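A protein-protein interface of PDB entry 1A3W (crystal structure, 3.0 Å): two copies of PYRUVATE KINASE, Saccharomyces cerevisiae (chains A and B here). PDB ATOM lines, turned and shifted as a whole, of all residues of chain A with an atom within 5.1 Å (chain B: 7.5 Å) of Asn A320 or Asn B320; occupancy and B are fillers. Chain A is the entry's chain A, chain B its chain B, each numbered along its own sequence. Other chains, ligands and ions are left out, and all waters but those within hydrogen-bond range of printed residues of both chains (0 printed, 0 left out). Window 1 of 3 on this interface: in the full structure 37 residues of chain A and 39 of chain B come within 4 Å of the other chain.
The side-chain amide nitrogen of Asn B320 lies close to the side-chain amino group of Lys A281 (3.3 Å). OG of Ser A316 sits at hydrogen-bond distance from OD1 of Asp B317 (3.3 Å). The side-chain hydroxyl (OG) of Ser B316 lies within hydrogen-bond range of the side-chain carboxylate (OD1) of Asp A317, at 3.3 Å. ND2 of Asn A320 sits close to NZ of Lys B281, at 3.2 Å. The side-chain amide oxygen (OD1) of Asn B320 sits close to the side-chain amide oxygen (OD1) of Asn A320 (3.1 Å).
Among the printed residues, merely in contact across the chains: Leu A277 with Val B315 (3.8 Å), Leu A277 with Ser B316 (3.6 Å), Leu A277 with Gly B319 (3.6 Å), Leu A277 with Asn B320 (3.9 Å), Lys A281 with Leu B323 (3.5 Å), Val A315 with Leu B277 (3.7 Å), Ser A316 with Leu B277 (3.5 Å), Asp A317 with Ala B313 (3.4 Å), Gly A319 with Leu B277 (3.5 Å), Asn A320 with Leu B277 (3.9 Å) and Leu A323 with Lys B281 (3.5 Å).
Leu A277 touches Val B315, and with the chains exchanged Val A315 touches Leu B277. Leu A277 touches Asn B320, and with the chains exchanged Asn A320 touches Leu B277. Lys A281 touches Asn B320, and with the chains exchanged Asn A320 touches Lys B281. Lys A281 touches Leu B323, and with the chains exchanged Leu A323 touches Lys B281. 13 positions are printed for both chains.
Along chain A the printed residues that touch a printed residue of chain B span positions 277 to 323. Printed residues of chain B that touch a printed residue of chain A: Leu B277, Lys B281, Ala B313, Val B315, Ser B316, Asp B317, Gly B319, Asn B320 and Leu B323. Hydrophobic or aromatic side chains of chain B that line the printed part of chain A: Leu B277, Ala B313 and Leu B323. Along chain B the printed residues that touch a printed residue of chain A span positions 277 to 323. Among the printed residues, 16 pairs touch across the chains. Among the printed residues, no Asp or Glu carboxylate lies within 4 Å of a Lys or Arg side-chain nitrogen of the other chain.
The side-chain amino group of Lys A281 lies within salt-bridge range of the side-chain carboxylate of Asp A324 (3.1 Å). OD1 of Asn A320 lies close to O of Ser A316, at 3.5 Å. OD1 of Asp B324 lies within salt-bridge range of NZ of Lys B281, 3.0 Å away. The backbone carbonyl oxygen (O) of Ala B313 lies within hydrogen-bond range of the side-chain hydroxyl (OG) of Ser B316. The side-chain amide oxygen (OD1) of Asn B320 sits close to the backbone carbonyl oxygen (O) of Ser B316 (3.4 Å).
Of chain B, only Leu B277, Lys B281 and Asn B320 come within 4 Å of Asn A320. Asn B320 touches three residues of chain A. Of chain B, only Leu B277 comes within 4 Å of Gly A319. Of the printed residues of chain A, Leu B323 touches Lys A281. Of the printed residues of chain A, Ala B313 touches Asp A317. Of the printed residues of chain B, Leu A323 touches Lys B281. The nearest residue of chain B that does not touch Asn A320 is Asp B324 (4.8 Å). The nearest residue of chain A that does not touch Asn B320 is Asp A324 (4.9 Å). The nearest printed residue of chain B that does not touch Asp A317 is Leu B277 (5.3 Å).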
ATOM      1  N   LEU A 277     -10.783  15.558  -5.079  1.00  0.00           N
ATOM      2  CA  LEU A 277     -10.911  15.283  -3.654  1.00  0.00           C
ATOM      3  C   LEU A 277     -10.118  14.038  -3.303  1.00  0.00           C
ATOM      4  O   LEU A 277      -9.586  13.920  -2.196  1.00  0.00           O
ATOM      5  CB  LEU A 277     -12.374  15.074  -3.265  1.00  0.00           C
ATOM      6  CG  LEU A 277     -12.567  14.528  -1.847  1.00  0.00           C
ATOM      7  CD1 LEU A 277     -13.499  15.427  -1.060  1.00  0.00           C
ATOM      8  CD2 LEU A 277     -13.122  13.121  -1.916  1.00  0.00           C
ATOM      9  N   LYS A 281      -5.922  13.936  -1.495  1.00  0.00           N
ATOM     10  CA  LYS A 281      -5.636  13.001  -0.409  1.00  0.00           C
ATOM     11  C   LYS A 281      -4.543  12.006  -0.751  1.00  0.00           C
ATOM     12  O   LYS A 281      -3.749  11.626   0.111  1.00  0.00           O
ATOM     13  CB  LYS A 281      -6.901  12.236  -0.028  1.00  0.00           C
ATOM     14  CG  LYS A 281      -7.926  13.071   0.706  1.00  0.00           C
ATOM     15  CD  LYS A 281      -9.181  12.276   0.995  1.00  0.00           C
ATOM     16  CE  LYS A 281      -9.887  12.812   2.225  1.00  0.00           C
ATOM     17  NZ  LYS A 281      -9.486  14.213   2.532  1.00  0.00           N
ATOM     18  N   VAL A 315     -13.168  27.103   5.600  1.00  0.00           N
ATOM     19  CA  VAL A 315     -12.320  26.751   6.735  1.00  0.00           C
ATOM     20  C   VAL A 315     -12.135  25.235   6.774  1.00  0.00           C
ATOM     21  O   VAL A 315     -11.050  24.739   7.079  1.00  0.00           O
ATOM     22  CB  VAL A 315     -12.910  27.258   8.090  1.00  0.00           C
ATOM     23  CG1 VAL A 315     -14.348  27.686   7.909  1.00  0.00           C
ATOM     24  CG2 VAL A 315     -12.806  26.182   9.151  1.00  0.00           C
ATOM     25  N   SER A 316     -13.193  24.502   6.450  1.00  0.00           N
ATOM     26  CA  SER A 316     -13.123  23.048   6.443  1.00  0.00           C
ATOM     27  C   SER A 316     -11.994  22.597   5.520  1.00  0.00           C
ATOM     28  O   SER A 316     -11.173  21.759   5.894  1.00  0.00           O
ATOM     29  CB  SER A 316     -14.449  22.454   5.965  1.00  0.00           C
ATOM     30  OG  SER A 316     -14.244  21.573   4.874  1.00  0.00           O
ATOM     31  N   ASP A 317     -11.957  23.160   4.314  1.00  0.00           N
ATOM     32  CA  ASP A 317     -10.924  22.808   3.346  1.00  0.00           C
ATOM     33  C   ASP A 317      -9.546  23.066   3.926  1.00  0.00           C
ATOM     34  O   ASP A 317      -8.656  22.215   3.856  1.00  0.00           O
ATOM     35  CB  ASP A 317     -11.079  23.622   2.065  1.00  0.00           C
ATOM     36  CG  ASP A 317     -10.029  23.268   1.027  1.00  0.00           C
ATOM     37  OD1 ASP A 317      -9.620  22.091   0.967  1.00  0.00           O
ATOM     38  OD2 ASP A 317      -9.611  24.164   0.270  1.00  0.00           O
ATOM     39  N   VAL A 318      -9.372  24.250   4.493  1.00  0.00           N
ATOM     40  CA  VAL A 318      -8.098  24.611   5.084  1.00  0.00           C
ATOM     41  C   VAL A 318      -7.662  23.497   6.026  1.00  0.00           C
ATOM     42  O   VAL A 318      -6.712  22.772   5.744  1.00  0.00           O
ATOM     43  CB  VAL A 318      -8.210  25.934   5.866  1.00  0.00           C
ATOM     44  CG1 VAL A 318      -7.033  26.093   6.803  1.00  0.00           C
ATOM     45  CG2 VAL A 318      -8.267  27.097   4.894  1.00  0.00           C
ATOM     46  N   GLY A 319      -8.382  23.354   7.131  1.00  0.00           N
ATOM     47  CA  GLY A 319      -8.055  22.338   8.116  1.00  0.00           C
ATOM     48  C   GLY A 319      -7.878  20.936   7.567  1.00  0.00           C
ATOM     49  O   GLY A 319      -6.891  20.266   7.873  1.00  0.00           O
ATOM     50  N   ASN A 320      -8.832  20.482   6.763  1.00  0.00           N
ATOM     51  CA  ASN A 320      -8.751  19.149   6.195  1.00  0.00           C
ATOM     52  C   ASN A 320      -7.481  18.987   5.378  1.00  0.00           C
ATOM     53  O   ASN A 320      -6.778  17.985   5.509  1.00  0.00           O
ATOM     54  CB  ASN A 320      -9.974  18.865   5.331  1.00  0.00           C
ATOM     55  CG  ASN A 320     -11.045  18.120   6.090  1.00  0.00           C
ATOM     56  OD1 ASN A 320     -12.223  18.467   6.028  1.00  0.00           O
ATOM     57  ND2 ASN A 320     -10.641  17.089   6.822  1.00  0.00           N
ATOM     58  N   ALA A 321      -7.187  19.971   4.535  1.00  0.00           N
ATOM     59  CA  ALA A 321      -5.974  19.922   3.723  1.00  0.00           C
ATOM     60  C   ALA A 321      -4.810  19.639   4.671  1.00  0.00           C
ATOM     61  O   ALA A 321      -3.955  18.806   4.391  1.00  0.00           O
ATOM     62  CB  ALA A 321      -5.762  21.246   3.000  1.00  0.00           C
ATOM     63  N   ILE A 322      -4.799  20.329   5.806  1.00  0.00           N
ATOM     64  CA  ILE A 322      -3.759  20.152   6.804  1.00  0.00           C
ATOM     65  C   ILE A 322      -3.850  18.748   7.394  1.00  0.00           C
ATOM     66  O   ILE A 322      -2.858  18.021   7.436  1.00  0.00           O
ATOM     67  CB  ILE A 322      -3.892  21.195   7.943  1.00  0.00           C
ATOM     68  CG1 ILE A 322      -3.282  22.525   7.494  1.00  0.00           C
ATOM     69  CG2 ILE A 322      -3.203  20.696   9.205  1.00  0.00           C
ATOM     70  CD1 ILE A 322      -3.842  23.743   8.203  1.00  0.00           C
ATOM     71  N   LEU A 323      -5.045  18.368   7.837  1.00  0.00           N
ATOM     72  CA  LEU A 323      -5.262  17.053   8.433  1.00  0.00           C
ATOM     73  C   LEU A 323      -4.939  15.906   7.485  1.00  0.00           C
ATOM     74  O   LEU A 323      -4.714  14.787   7.931  1.00  0.00           O
ATOM     75  CB  LEU A 323      -6.703  16.924   8.920  1.00  0.00           C
ATOM     76  CG  LEU A 323      -6.942  17.456  10.333  1.00  0.00           C
ATOM     77  CD1 LEU A 323      -8.402  17.787  10.513  1.00  0.00           C
ATOM     78  CD2 LEU A 323      -6.508  16.418  11.351  1.00  0.00           C
ATOM     79  N   ASP A 324      -4.923  16.182   6.183  1.00  0.00           N
ATOM     80  CA  ASP A 324      -4.606  15.148   5.202  1.00  0.00           C
ATOM     81  C   ASP A 324      -3.122  14.858   5.313  1.00  0.00           C
ATOM     82  O   ASP A 324      -2.682  13.717   5.159  1.00  0.00           O
ATOM     83  CB  ASP A 324      -4.912  15.623   3.783  1.00  0.00           C
ATOM     84  CG  ASP A 324      -6.381  15.924   3.573  1.00  0.00           C
ATOM     85  OD1 ASP A 324      -7.224  15.313   4.270  1.00  0.00           O
ATOM     86  OD2 ASP A 324      -6.689  16.773   2.708  1.00  0.00           O
ATOM     87  N   GLY A 325      -2.357  15.911   5.590  1.00  0.00           N
ATOM     88  CA  GLY A 325      -0.918  15.784   5.726  1.00  0.00           C
ATOM     89  C   GLY A 325      -0.195  16.937   5.056  1.00  0.00           C
ATOM     90  O   GLY A 325       1.036  16.968   5.010  1.00  0.00           O
ATOM     91  N   LEU B 277     -14.667  23.392  12.619  1.00  0.00           N
ATOM     92  CA  LEU B 277     -13.996  22.309  11.910  1.00  0.00           C
ATOM     93  C   LEU B 277     -13.799  21.133  12.846  1.00  0.00           C
ATOM     94  O   LEU B 277     -13.832  19.978  12.429  1.00  0.00           O
ATOM     95  CB  LEU B 277     -12.641  22.765  11.378  1.00  0.00           C
ATOM     96  CG  LEU B 277     -11.770  21.630  10.837  1.00  0.00           C
ATOM     97  CD1 LEU B 277     -11.318  21.946   9.425  1.00  0.00           C
ATOM     98  CD2 LEU B 277     -10.584  21.433  11.751  1.00  0.00           C
ATOM     99  N   GLN B 280     -17.547  19.923  14.247  1.00  0.00           N
ATOM    100  CA  GLN B 280     -18.211  19.078  13.263  1.00  0.00           C
ATOM    101  C   GLN B 280     -17.700  17.654  13.452  1.00  0.00           C
ATOM    102  O   GLN B 280     -18.411  16.800  13.969  1.00  0.00           O
ATOM    103  CB  GLN B 280     -17.902  19.569  11.847  1.00  0.00           C
ATOM    104  CG  GLN B 280     -18.085  18.529  10.762  1.00  0.00           C
ATOM    105  CD  GLN B 280     -18.050  19.140   9.370  1.00  0.00           C
ATOM    106  OE1 GLN B 280     -17.608  18.513   8.403  1.00  0.00           O
ATOM    107  NE2 GLN B 280     -18.517  20.376   9.262  1.00  0.00           N
ATOM    108  N   LYS B 281     -16.452  17.419  13.052  1.00  0.00           N
ATOM    109  CA  LYS B 281     -15.817  16.109  13.169  1.00  0.00           C
ATOM    110  C   LYS B 281     -16.205  15.366  14.440  1.00  0.00           C
ATOM    111  O   LYS B 281     -16.357  14.147  14.431  1.00  0.00           O
ATOM    112  CB  LYS B 281     -14.298  16.259  13.125  1.00  0.00           C
ATOM    113  CG  LYS B 281     -13.757  16.600  11.753  1.00  0.00           C
ATOM    114  CD  LYS B 281     -12.253  16.784  11.784  1.00  0.00           C
ATOM    115  CE  LYS B 281     -11.640  16.512  10.419  1.00  0.00           C
ATOM    116  NZ  LYS B 281     -12.643  16.568   9.321  1.00  0.00           N
ATOM    117  N   ILE B 284     -20.481  14.796  14.444  1.00  0.00           N
ATOM    118  CA  ILE B 284     -20.748  13.789  13.426  1.00  0.00           C
ATOM    119  C   ILE B 284     -20.307  12.422  13.925  1.00  0.00           C
ATOM    120  O   ILE B 284     -20.994  11.431  13.706  1.00  0.00           O
ATOM    121  CB  ILE B 284     -19.996  14.100  12.119  1.00  0.00           C
ATOM    122  CG1 ILE B 284     -20.855  14.992  11.226  1.00  0.00           C
ATOM    123  CG2 ILE B 284     -19.634  12.800  11.396  1.00  0.00           C
ATOM    124  CD1 ILE B 284     -20.355  15.081   9.810  1.00  0.00           C
ATOM    125  N   CYS B 296     -24.935  17.245   7.673  1.00  0.00           N
ATOM    126  CA  CYS B 296     -23.996  18.358   7.616  1.00  0.00           C
ATOM    127  C   CYS B 296     -24.609  19.385   6.671  1.00  0.00           C
ATOM    128  O   CYS B 296     -25.025  19.026   5.572  1.00  0.00           O
ATOM    129  CB  CYS B 296     -22.657  17.878   7.062  1.00  0.00           C
ATOM    130  SG  CYS B 296     -21.331  19.061   7.247  1.00  0.00           S
ATOM    131  N   MET B 300     -22.297  24.332   1.731  1.00  0.00           N
ATOM    132  CA  MET B 300     -21.565  23.176   1.218  1.00  0.00           C
ATOM    133  C   MET B 300     -21.231  23.385  -0.253  1.00  0.00           C
ATOM    134  O   MET B 300     -20.461  22.631  -0.843  1.00  0.00           O
ATOM    135  CB  MET B 300     -22.394  21.903   1.382  1.00  0.00           C
ATOM    136  CG  MET B 300     -22.673  21.545   2.823  1.00  0.00           C
ATOM    137  SD  MET B 300     -22.599  19.781   3.120  1.00  0.00           S
ATOM    138  CE  MET B 300     -20.835  19.494   3.002  1.00  0.00           C
ATOM    139  N   ALA B 313     -12.407  24.157  -2.653  1.00  0.00           N
ATOM    140  CA  ALA B 313     -12.730  24.059  -1.237  1.00  0.00           C
ATOM    141  C   ALA B 313     -14.132  23.517  -1.030  1.00  0.00           C
ATOM    142  O   ALA B 313     -14.395  22.797  -0.063  1.00  0.00           O
ATOM    143  CB  ALA B 313     -12.599  25.430  -0.578  1.00  0.00           C
ATOM    144  N   GLU B 314     -15.032  23.863  -1.943  1.00  0.00           N
ATOM    145  CA  GLU B 314     -16.417  23.423  -1.849  1.00  0.00           C
ATOM    146  C   GLU B 314     -16.582  21.914  -1.951  1.00  0.00           C
ATOM    147  O   GLU B 314     -17.060  21.280  -1.009  1.00  0.00           O
ATOM    148  CB  GLU B 314     -17.256  24.116  -2.915  1.00  0.00           C
ATOM    149  CG  GLU B 314     -18.298  25.052  -2.333  1.00  0.00           C
ATOM    150  CD  GLU B 314     -18.326  26.397  -3.025  1.00  0.00           C
ATOM    151  OE1 GLU B 314     -18.117  26.429  -4.257  1.00  0.00           O
ATOM    152  OE2 GLU B 314     -18.557  27.417  -2.341  1.00  0.00           O
ATOM    153  N   VAL B 315     -16.192  21.338  -3.086  1.00  0.00           N
ATOM    154  CA  VAL B 315     -16.307  19.891  -3.265  1.00  0.00           C
ATOM    155  C   VAL B 315     -15.575  19.170  -2.128  1.00  0.00           C
ATOM    156  O   VAL B 315     -16.034  18.145  -1.629  1.00  0.00           O
ATOM    157  CB  VAL B 315     -15.736  19.428  -4.641  1.00  0.00           C
ATOM    158  CG1 VAL B 315     -14.928  20.536  -5.278  1.00  0.00           C
ATOM    159  CG2 VAL B 315     -14.888  18.187  -4.472  1.00  0.00           C
ATOM    160  N   SER B 316     -14.439  19.718  -1.713  1.00  0.00           N
ATOM    161  CA  SER B 316     -13.674  19.134  -0.622  1.00  0.00           C
ATOM    162  C   SER B 316     -14.562  19.011   0.614  1.00  0.00           C
ATOM    163  O   SER B 316     -14.603  17.960   1.252  1.00  0.00           O
ATOM    164  CB  SER B 316     -12.463  20.006  -0.290  1.00  0.00           C
ATOM    165  OG  SER B 316     -12.451  20.344   1.088  1.00  0.00           O
ATOM    166  N   ASP B 317     -15.270  20.088   0.947  1.00  0.00           N
ATOM    167  CA  ASP B 317     -16.156  20.090   2.108  1.00  0.00           C
ATOM    168  C   ASP B 317     -17.200  18.990   1.985  1.00  0.00           C
ATOM    169  O   ASP B 317     -17.441  18.226   2.927  1.00  0.00           O
ATOM    170  CB  ASP B 317     -16.867  21.437   2.242  1.00  0.00           C
ATOM    171  CG  ASP B 317     -17.771  21.497   3.463  1.00  0.00           C
ATOM    172  OD1 ASP B 317     -17.433  20.873   4.491  1.00  0.00           O
ATOM    173  OD2 ASP B 317     -18.820  22.168   3.399  1.00  0.00           O
ATOM    174  N   VAL B 318     -17.827  18.922   0.820  1.00  0.00           N
ATOM    175  CA  VAL B 318     -18.840  17.915   0.577  1.00  0.00           C
ATOM    176  C   VAL B 318     -18.277  16.549   0.949  1.00  0.00           C
ATOM    177  O   VAL B 318     -18.696  15.942   1.937  1.00  0.00           O
ATOM    178  CB  VAL B 318     -19.262  17.911  -0.901  1.00  0.00           C
ATOM    179  CG1 VAL B 318     -19.991  16.625  -1.239  1.00  0.00           C
ATOM    180  CG2 VAL B 318     -20.146  19.104  -1.178  1.00  0.00           C
ATOM    181  N   GLY B 319     -17.307  16.088   0.160  1.00  0.00           N
ATOM    182  CA  GLY B 319     -16.693  14.793   0.391  1.00  0.00           C
ATOM    183  C   GLY B 319     -16.208  14.561   1.809  1.00  0.00           C
ATOM    184  O   GLY B 319     -16.513  13.537   2.417  1.00  0.00           O
ATOM    185  N   ASN B 320     -15.448  15.508   2.343  1.00  0.00           N
ATOM    186  CA  ASN B 320     -14.924  15.372   3.693  1.00  0.00           C
ATOM    187  C   ASN B 320     -16.050  15.192   4.694  1.00  0.00           C
ATOM    188  O   ASN B 320     -15.979  14.328   5.566  1.00  0.00           O
ATOM    189  CB  ASN B 320     -14.083  16.593   4.058  1.00  0.00           C
ATOM    190  CG  ASN B 320     -12.609  16.361   3.828  1.00  0.00           C
ATOM    191  OD1 ASN B 320     -11.918  17.193   3.237  1.00  0.00           O
ATOM    192  ND2 ASN B 320     -12.116  15.216   4.291  1.00  0.00           N
ATOM    193  N   ALA B 321     -17.087  16.015   4.565  1.00  0.00           N
ATOM    194  CA  ALA B 321     -18.236  15.926   5.454  1.00  0.00           C
ATOM    195  C   ALA B 321     -18.692  14.474   5.441  1.00  0.00           C
ATOM    196  O   ALA B 321     -18.960  13.884   6.487  1.00  0.00           O
ATOM    197  CB  ALA B 321     -19.341  16.829   4.958  1.00  0.00           C
ATOM    198  N   ILE B 322     -18.757  13.899   4.245  1.00  0.00           N
ATOM    199  CA  ILE B 322     -19.160  12.508   4.077  1.00  0.00           C
ATOM    200  C   ILE B 322     -18.124  11.589   4.720  1.00  0.00           C
ATOM    201  O   ILE B 322     -18.467  10.730   5.534  1.00  0.00           O
ATOM    202  CB  ILE B 322     -19.306  12.142   2.575  1.00  0.00           C
ATOM    203  CG1 ILE B 322     -20.650  12.643   2.047  1.00  0.00           C
ATOM    204  CG2 ILE B 322     -19.216  10.643   2.385  1.00  0.00           C
ATOM    205  CD1 ILE B 322     -20.676  12.910   0.556  1.00  0.00           C
ATOM    206  N   LEU B 323     -16.857  11.781   4.360  1.00  0.00           N
ATOM    207  CA  LEU B 323     -15.770  10.964   4.901  1.00  0.00           C
ATOM    208  C   LEU B 323     -15.659  11.045   6.417  1.00  0.00           C
ATOM    209  O   LEU B 323     -15.067  10.172   7.038  1.00  0.00           O
ATOM    210  CB  LEU B 323     -14.431  11.367   4.279  1.00  0.00           C
ATOM    211  CG  LEU B 323     -14.125  10.678   2.951  1.00  0.00           C
ATOM    212  CD1 LEU B 323     -13.133  11.490   2.146  1.00  0.00           C
ATOM    213  CD2 LEU B 323     -13.588   9.296   3.229  1.00  0.00           C
ATOM    214  N   ASP B 324     -16.213  12.095   7.015  1.00  0.00           N
ATOM    215  CA  ASP B 324     -16.159  12.233   8.465  1.00  0.00           C
ATOM    216  C   ASP B 324     -17.112  11.213   9.058  1.00  0.00           C
ATOM    217  O   ASP B 324     -16.863  10.652  10.126  1.00  0.00           O
ATOM    218  CB  ASP B 324     -16.594  13.633   8.904  1.00  0.00           C
ATOM    219  CG  ASP B 324     -15.698  14.721   8.364  1.00  0.00           C
ATOM    220  OD1 ASP B 324     -14.497  14.466   8.145  1.00  0.00           O
ATOM    221  OD2 ASP B 324     -16.203  15.840   8.156  1.00  0.00           O
ATOM    222  N   GLY B 325     -18.212  10.985   8.346  1.00  0.00           N
ATOM    223  CA  GLY B 325     -19.210  10.035   8.795  1.00  0.00           C
ATOM    224  C   GLY B 325     -20.614  10.561   8.579  1.00  0.00           C
ATOM    225  O   GLY B 325     -21.594   9.917   8.951  1.00  0.00           O
ATOM    226  N   ALA B 326     -20.708  11.736   7.971  1.00  0.00           N
ATOM    227  CA  ALA B 326     -21.996  12.361   7.705  1.00  0.00           C
ATOM    228  C   ALA B 326     -22.959  11.418   6.993  1.00  0.00           C
ATOM    229  O   ALA B 326     -22.577  10.686   6.082  1.00  0.00           O
ATOM    230  CB  ALA B 326     -21.802  13.619   6.878  1.00  0.00           C
ATOM    231  N   VAL B 329     -26.006  15.338   3.570  1.00  0.00           N
ATOM    232  CA  VAL B 329     -25.393  16.605   3.200  1.00  0.00           C
ATOM    233  C   VAL B 329     -26.431  17.423   2.427  1.00  0.00           C
ATOM    234  O   VAL B 329     -26.756  17.117   1.278  1.00  0.00           O
ATOM    235  CB  VAL B 329     -24.144  16.379   2.318  1.00  0.00           C
ATOM    236  CG1 VAL B 329     -23.019  15.791   3.154  1.00  0.00           C
ATOM    237  CG2 VAL B 329     -24.482  15.448   1.165  1.00  0.00           C
ATOM    238  N   THR B 351     -19.612  14.159  -6.134  1.00  0.00           N
ATOM    239  CA  THR B 351     -18.590  14.248  -5.104  1.00  0.00           C
ATOM    240  C   THR B 351     -18.842  13.157  -4.080  1.00  0.00           C
ATOM    241  O   THR B 351     -17.913  12.526  -3.589  1.00  0.00           O
ATOM    242  CB  THR B 351     -18.639  15.606  -4.389  1.00  0.00           C
ATOM    243  OG1 THR B 351     -18.386  16.649  -5.338  1.00  0.00           O
ATOM    244  CG2 THR B 351     -17.605  15.665  -3.279  1.00  0.00           C
ATOM    245  N   ALA B 355     -16.278  10.323  -2.414  1.00  0.00           N
ATOM    246  CA  ALA B 355     -16.081  10.363  -0.970  1.00  0.00           C
ATOM    247  C   ALA B 355     -16.204   8.979  -0.351  1.00  0.00           C
ATOM    248  O   ALA B 355     -15.249   8.469   0.229  1.00  0.00           O
ATOM    249  CB  ALA B 355     -17.086  11.306  -0.331  1.00  0.00           C
ATOM    250  N   ARG B 437     -27.478   6.646   5.685  1.00  0.00           N
ATOM    251  CA  ARG B 437     -26.597   6.367   4.560  1.00  0.00           C
ATOM    252  C   ARG B 437     -26.567   4.888   4.210  1.00  0.00           C
ATOM    253  O   ARG B 437     -26.507   4.033   5.091  1.00  0.00           O
ATOM    254  CB  ARG B 437     -25.177   6.847   4.872  1.00  0.00           C
ATOM    255  CG  ARG B 437     -24.218   6.739   3.698  1.00  0.00           C
ATOM    256  CD  ARG B 437     -22.779   6.567   4.155  1.00  0.00           C
ATOM    257  NE  ARG B 437     -22.287   7.755   4.843  1.00  0.00           N
ATOM    258  CZ  ARG B 437     -21.007   7.987   5.111  1.00  0.00           C
ATOM    259  NH1 ARG B 437     -20.082   7.109   4.751  1.00  0.00           N
ATOM    260  NH2 ARG B 437     -20.649   9.097   5.744  1.00  0.00           N
